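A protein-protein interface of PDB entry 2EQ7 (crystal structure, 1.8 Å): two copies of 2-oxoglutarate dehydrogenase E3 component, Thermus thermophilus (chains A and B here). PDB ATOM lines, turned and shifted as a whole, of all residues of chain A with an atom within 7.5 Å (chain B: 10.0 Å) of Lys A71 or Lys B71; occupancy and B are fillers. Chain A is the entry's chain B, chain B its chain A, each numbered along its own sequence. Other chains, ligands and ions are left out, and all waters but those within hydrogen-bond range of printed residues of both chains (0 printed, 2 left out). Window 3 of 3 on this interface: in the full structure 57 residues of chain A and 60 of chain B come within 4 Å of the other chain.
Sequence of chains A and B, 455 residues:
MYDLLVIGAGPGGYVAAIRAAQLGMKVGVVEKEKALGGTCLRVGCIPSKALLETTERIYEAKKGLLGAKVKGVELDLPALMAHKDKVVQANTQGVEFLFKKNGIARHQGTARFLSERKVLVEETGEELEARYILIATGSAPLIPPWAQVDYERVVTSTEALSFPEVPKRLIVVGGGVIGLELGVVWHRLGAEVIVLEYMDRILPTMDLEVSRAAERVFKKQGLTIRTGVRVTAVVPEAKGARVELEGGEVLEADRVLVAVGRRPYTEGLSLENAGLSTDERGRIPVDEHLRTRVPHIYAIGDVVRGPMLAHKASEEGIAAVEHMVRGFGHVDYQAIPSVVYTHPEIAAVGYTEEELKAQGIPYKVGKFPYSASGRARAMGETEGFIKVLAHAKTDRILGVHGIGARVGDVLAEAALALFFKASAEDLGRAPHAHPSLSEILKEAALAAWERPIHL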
ATOM      1  N   ALA A  61      21.294 -17.024  18.728  1.00  0.00           N
ATOM      2  CA  ALA A  61      20.103 -17.294  19.528  1.00  0.00           C
ATOM      3  C   ALA A  61      20.457 -17.265  21.015  1.00  0.00           C
ATOM      4  O   ALA A  61      19.660 -16.822  21.846  1.00  0.00           O
ATOM      5  CB  ALA A  61      19.510 -18.654  19.153  1.00  0.00           C
ATOM      6  N   LYS A  69      12.753 -12.716  23.180  1.00  0.00           N
ATOM      7  CA  LYS A  69      13.383 -13.314  24.342  1.00  0.00           C
ATOM      8  C   LYS A  69      13.370 -14.820  24.132  1.00  0.00           C
ATOM      9  O   LYS A  69      12.358 -15.389  23.723  1.00  0.00           O
ATOM     10  CB  LYS A  69      12.609 -12.965  25.615  1.00  0.00           C
ATOM     11  CG  LYS A  69      12.543 -11.478  25.921  1.00  0.00           C
ATOM     12  CD  LYS A  69      11.716 -11.220  27.172  1.00  0.00           C
ATOM     13  CE  LYS A  69      11.682  -9.740  27.520  1.00  0.00           C
ATOM     14  NZ  LYS A  69      13.045  -9.214  27.820  1.00  0.00           N
ATOM     15  N   VAL A  70      14.502 -15.460  24.389  1.00  0.00           N
ATOM     16  CA  VAL A  70      14.604 -16.905  24.244  1.00  0.00           C
ATOM     17  C   VAL A  70      14.935 -17.475  25.616  1.00  0.00           C
ATOM     18  O   VAL A  70      15.988 -17.174  26.180  1.00  0.00           O
ATOM     19  CB  VAL A  70      15.716 -17.292  23.252  1.00  0.00           C
ATOM     20  CG1 VAL A  70      15.751 -18.801  23.075  1.00  0.00           C
ATOM     21  CG2 VAL A  70      15.482 -16.603  21.917  1.00  0.00           C
ATOM     22  N   LYS A  71      14.032 -18.285  26.157  1.00  0.00           N
ATOM     23  CA  LYS A  71      14.242 -18.871  27.473  1.00  0.00           C
ATOM     24  C   LYS A  71      15.433 -19.818  27.502  1.00  0.00           C
ATOM     25  O   LYS A  71      16.167 -19.867  28.488  1.00  0.00           O
ATOM     26  CB  LYS A  71      12.978 -19.598  27.937  1.00  0.00           C
ATOM     27  CG  LYS A  71      11.826 -18.654  28.237  1.00  0.00           C
ATOM     28  CD  LYS A  71      10.593 -19.391  28.725  1.00  0.00           C
ATOM     29  CE  LYS A  71       9.491 -18.409  29.097  1.00  0.00           C
ATOM     30  NZ  LYS A  71       9.151 -17.496  27.963  1.00  0.00           N
ATOM     31  N   GLY A  72      15.637 -20.561  26.420  1.00  0.00           N
ATOM     32  CA  GLY A  72      16.756 -21.480  26.393  1.00  0.00           C
ATOM     33  C   GLY A  72      17.119 -22.035  25.032  1.00  0.00           C
ATOM     34  O   GLY A  72      16.270 -22.204  24.158  1.00  0.00           O
ATOM     35  N   VAL A  73      18.404 -22.309  24.857  1.00  0.00           N
ATOM     36  CA  VAL A  73      18.910 -22.876  23.619  1.00  0.00           C
ATOM     37  C   VAL A  73      19.712 -24.102  24.022  1.00  0.00           C
ATOM     38  O   VAL A  73      20.713 -23.988  24.731  1.00  0.00           O
ATOM     39  CB  VAL A  73      19.832 -21.894  22.880  1.00  0.00           C
ATOM     40  CG1 VAL A  73      20.340 -22.530  21.597  1.00  0.00           C
ATOM     41  CG2 VAL A  73      19.083 -20.604  22.579  1.00  0.00           C
ATOM     42  N   GLU A  74      19.260 -25.271  23.585  1.00  0.00           N
ATOM     43  CA  GLU A  74      19.941 -26.515  23.920  1.00  0.00           C
ATOM     44  C   GLU A  74      20.598 -27.137  22.695  1.00  0.00           C
ATOM     45  O   GLU A  74      19.936 -27.435  21.705  1.00  0.00           O
ATOM     46  CB  GLU A  74      18.951 -27.510  24.531  1.00  0.00           C
ATOM     47  CG  GLU A  74      19.610 -28.748  25.115  1.00  0.00           C
ATOM     48  CD  GLU A  74      18.605 -29.734  25.675  1.00  0.00           C
ATOM     49  OE1 GLU A  74      17.754 -29.318  26.492  1.00  0.00           O
ATOM     50  OE2 GLU A  74      18.670 -30.925  25.304  1.00  0.00           O
ATOM     51  N   ALA B  61      14.127 -19.023  14.612  1.00  0.00           N
ATOM     52  CA  ALA B  61      14.308 -19.561  15.954  1.00  0.00           C
ATOM     53  C   ALA B  61      13.045 -20.326  16.354  1.00  0.00           C
ATOM     54  O   ALA B  61      13.125 -21.396  16.958  1.00  0.00           O
ATOM     55  CB  ALA B  61      14.578 -18.434  16.943  1.00  0.00           C
ATOM     56  N   LYS B  62      11.884 -19.773  16.011  1.00  0.00           N
ATOM     57  CA  LYS B  62      10.609 -20.415  16.327  1.00  0.00           C
ATOM     58  C   LYS B  62      10.430 -21.718  15.552  1.00  0.00           C
ATOM     59  O   LYS B  62      10.003 -22.727  16.115  1.00  0.00           O
ATOM     60  CB  LYS B  62       9.436 -19.481  16.003  1.00  0.00           C
ATOM     61  CG  LYS B  62       9.307 -18.272  16.915  1.00  0.00           C
ATOM     62  CD  LYS B  62       8.054 -17.469  16.570  1.00  0.00           C
ATOM     63  CE  LYS B  62       7.866 -16.289  17.513  1.00  0.00           C
ATOM     64  NZ  LYS B  62       6.585 -15.570  17.258  1.00  0.00           N
ATOM     65  N   LYS B  63      10.748 -21.695  14.260  1.00  0.00           N
ATOM     66  CA  LYS B  63      10.613 -22.887  13.425  1.00  0.00           C
ATOM     67  C   LYS B  63      11.569 -23.975  13.901  1.00  0.00           C
ATOM     68  O   LYS B  63      11.241 -25.163  13.869  1.00  0.00           O
ATOM     69  CB  LYS B  63      10.913 -22.558  11.959  1.00  0.00           C
ATOM     70  CG  LYS B  63       9.953 -21.565  11.313  1.00  0.00           C
ATOM     71  CD  LYS B  63       8.525 -22.095  11.268  1.00  0.00           C
ATOM     72  CE  LYS B  63       8.415 -23.351  10.413  1.00  0.00           C
ATOM     73  NZ  LYS B  63       8.779 -23.102   8.988  1.00  0.00           N
ATOM     74  N   GLY B  64      12.751 -23.557  14.343  1.00  0.00           N
ATOM     75  CA  GLY B  64      13.743 -24.503  14.817  1.00  0.00           C
ATOM     76  C   GLY B  64      15.069 -24.320  14.103  1.00  0.00           C
ATOM     77  O   GLY B  64      15.108 -24.078  12.894  1.00  0.00           O
ATOM     78  N   LEU B  65      16.159 -24.431  14.853  1.00  0.00           N
ATOM     79  CA  LEU B  65      17.494 -24.274  14.291  1.00  0.00           C
ATOM     80  C   LEU B  65      18.180 -25.628  14.184  1.00  0.00           C
ATOM     81  O   LEU B  65      18.085 -26.453  15.093  1.00  0.00           O
ATOM     82  CB  LEU B  65      18.334 -23.349  15.173  1.00  0.00           C
ATOM     83  CG  LEU B  65      17.794 -21.937  15.412  1.00  0.00           C
ATOM     84  CD1 LEU B  65      18.722 -21.202  16.365  1.00  0.00           C
ATOM     85  CD2 LEU B  65      17.674 -21.184  14.099  1.00  0.00           C
ATOM     86  N   ALA B  68      20.050 -27.673  17.155  1.00  0.00           N
ATOM     87  CA  ALA B  68      19.669 -27.146  18.457  1.00  0.00           C
ATOM     88  C   ALA B  68      18.184 -27.271  18.733  1.00  0.00           C
ATOM     89  O   ALA B  68      17.392 -27.583  17.844  1.00  0.00           O
ATOM     90  CB  ALA B  68      20.093 -25.688  18.578  1.00  0.00           C
ATOM     91  N   LYS B  69      17.822 -27.031  19.986  1.00  0.00           N
ATOM     92  CA  LYS B  69      16.437 -27.082  20.415  1.00  0.00           C
ATOM     93  C   LYS B  69      16.156 -25.803  21.187  1.00  0.00           C
ATOM     94  O   LYS B  69      16.694 -25.595  22.274  1.00  0.00           O
ATOM     95  CB  LYS B  69      16.197 -28.307  21.302  1.00  0.00           C
ATOM     96  CG  LYS B  69      16.404 -29.634  20.578  1.00  0.00           C
ATOM     97  CD  LYS B  69      16.099 -30.830  21.469  1.00  0.00           C
ATOM     98  CE  LYS B  69      17.070 -30.924  22.636  1.00  0.00           C
ATOM     99  NZ  LYS B  69      16.812 -32.129  23.474  1.00  0.00           N
ATOM    100  N   VAL B  70      15.337 -24.932  20.611  1.00  0.00           N
ATOM    101  CA  VAL B  70      14.986 -23.681  21.268  1.00  0.00           C
ATOM    102  C   VAL B  70      13.733 -23.924  22.101  1.00  0.00           C
ATOM    103  O   VAL B  70      12.653 -24.165  21.558  1.00  0.00           O
ATOM    104  CB  VAL B  70      14.723 -22.565  20.240  1.00  0.00           C
ATOM    105  CG1 VAL B  70      14.465 -21.249  20.956  1.00  0.00           C
ATOM    106  CG2 VAL B  70      15.917 -22.433  19.309  1.00  0.00           C
ATOM    107  N   LYS B  71      13.889 -23.866  23.420  1.00  0.00           N
ATOM    108  CA  LYS B  71      12.791 -24.109  24.350  1.00  0.00           C
ATOM    109  C   LYS B  71      11.605 -23.185  24.117  1.00  0.00           C
ATOM    110  O   LYS B  71      10.460 -23.635  24.035  1.00  0.00           O
ATOM    111  CB  LYS B  71      13.285 -23.966  25.792  1.00  0.00           C
ATOM    112  CG  LYS B  71      12.406 -24.673  26.815  1.00  0.00           C
ATOM    113  CD  LYS B  71      13.063 -24.720  28.187  1.00  0.00           C
ATOM    114  CE  LYS B  71      13.082 -23.352  28.840  1.00  0.00           C
ATOM    115  NZ  LYS B  71      11.700 -22.831  29.047  1.00  0.00           N
ATOM    116  N   GLY B  72      11.878 -21.890  24.012  1.00  0.00           N
ATOM    117  CA  GLY B  72      10.804 -20.946  23.788  1.00  0.00           C
ATOM    118  C   GLY B  72      11.280 -19.656  23.155  1.00  0.00           C
ATOM    119  O   GLY B  72      12.439 -19.264  23.302  1.00  0.00           O
ATOM    120  N   VAL B  73      10.378 -19.002  22.436  1.00  0.00           N
ATOM    121  CA  VAL B  73      10.678 -17.737  21.784  1.00  0.00           C
ATOM    122  C   VAL B  73       9.505 -16.809  22.068  1.00  0.00           C
ATOM    123  O   VAL B  73       8.380 -17.072  21.642  1.00  0.00           O
ATOM    124  CB  VAL B  73      10.852 -17.916  20.261  1.00  0.00           C
ATOM    125  CG1 VAL B  73      11.007 -16.563  19.591  1.00  0.00           C
ATOM    126  CG2 VAL B  73      12.073 -18.782  19.981  1.00  0.00           C
ATOM    127  N   GLU B  74       9.772 -15.735  22.802  1.00  0.00           N
ATOM    128  CA  GLU B  74       8.738 -14.774  23.166  1.00  0.00           C
ATOM    129  C   GLU B  74       8.966 -13.420  22.503  1.00  0.00           C
ATOM    130  O   GLU B  74      10.016 -12.805  22.667  1.00  0.00           O
ATOM    131  CB  GLU B  74       8.702 -14.609  24.688  1.00  0.00           C
ATOM    132  CG  GLU B  74       7.641 -13.644  25.195  1.00  0.00           C
ATOM    133  CD  GLU B  74       7.554 -13.622  26.714  1.00  0.00           C
ATOM    134  OE1 GLU B  74       7.256 -14.681  27.311  1.00  0.00           O
ATOM    135  OE2 GLU B  74       7.785 -12.547  27.310  1.00  0.00           O
ATOM    136  N   LEU B  75       7.970 -12.956  21.759  1.00  0.00           N
ATOM    137  CA  LEU B  75       8.078 -11.674  21.080  1.00  0.00           C
ATOM    138  C   LEU B  75       8.044 -10.501  22.052  1.00  0.00           C
ATOM    139  O   LEU B  75       7.269 -10.490  23.008  1.00  0.00           O
ATOM    140  CB  LEU B  75       6.940 -11.509  20.071  1.00  0.00           C
ATOM    141  CG  LEU B  75       6.868 -10.148  19.370  1.00  0.00           C
ATOM    142  CD1 LEU B  75       8.092  -9.962  18.478  1.00  0.00           C
ATOM    143  CD2 LEU B  75       5.582 -10.059  18.551  1.00  0.00           C
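Lys A69 touches Val B73, and with the chains exchanged Val A73 touches Lys B69. Lys B71 touches its own counterpart, Lys A71. Lys A71 touches Gly B72, and with the chains exchanged Gly A72 touches Lys B71. Lys A71 touches Glu B74, but with the chains exchanged Glu A74 does not touch Lys B71 (5.6 Å). 7 positions are printed for both chains.
Of the printed residues of chain B, Lys A71 touches Lys B71 (3.6 Å), Gly B72 (3.4 Å) and Glu B74 (3.5 Å). Lys B71 touches just these residues of chain A: Lys A71 (3.6 Å) and Gly A72 (3.0 Å). Of chain B, only Val B70 and Gly B72 come within 4 Å of Val A70. Gly A72 touches just these residues of chain B: Lys B69 (3.9 Å), Val B70 (3.5 Å) and Lys B71 (3.0 Å). Of the printed residues of chain A, Gly B72 touches Lys A69, Val A70 and Lys A71. Of the printed residues of chain B, Lys A69 touches Gly B72, Val B73 and Glu B74. Of the printed residues of chain A, Val B70 touches Val A70 (3.5 Å) and Gly A72 (3.5 Å). Of the printed residues of chain A, Glu B74 touches Lys A69 and Lys A71. Gly B64 touches none of the printed residues of chain A. The nearest residue of chain B that does not touch Lys A71 is Val B73 (5.3 Å). The nearest residue of chain A that does not touch Lys B71 is Val A73 (5.0 Å). The nearest printed residue of chain A that does not touch Gly B72 is Gly A72 (4.4 Å).
Among the printed residues, pairs that only touch across the chains: Glu A74 with Ala B68 (3.3 Å), Val A70 with Gly B72 (3.3 Å), Lys A69 with Val B73 (3.5 Å), Val A70 with Val B70 (3.5 Å), Gly A72 with Val B70 (3.5 Å), Lys A71 with Lys B71 (3.6 Å), Val A73 with Lys B69 (3.8 Å), Ala A61 with Leu B65 (3.9 Å), Lys A69 with Gly B72 (3.9 Å) and Gly A72 with Lys B69 (3.9 Å).
Printed residues of chain B that touch a printed residue of chain A: Leu B65, Ala B68, Lys B69, Val B70, Lys B71, Gly B72, Val B73 and Glu B74. Among the printed residues, 15 pairs touch across the chains. Among the printed residues, Asp or Glu carboxylates within 4 Å of a Lys or Arg side-chain nitrogen of the other chain: Lys A71 with Glu B74 and Glu A74 with Lys B69.
N of Lys B71 sits at hydrogen-bond distance from O of Gly A72 (3.0 Å). N of Glu B74 lies within hydrogen-bond range of O of Lys A69, at 2.8 Å. The side-chain carboxylate (OE1) of Glu B74 is in salt-bridge range of the side-chain amino group (NZ) of Lys A71, at 3.5 Å. The backbone carbonyl oxygen (O) of Gly B72 lies within hydrogen-bond range of the backbone NH (N) of Lys A71, at 3.4 Å. The side-chain amino group (NZ) of Lys B69 is in salt-bridge range of the side-chain carboxylate (OE2) of Glu A74 (2.9 Å).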
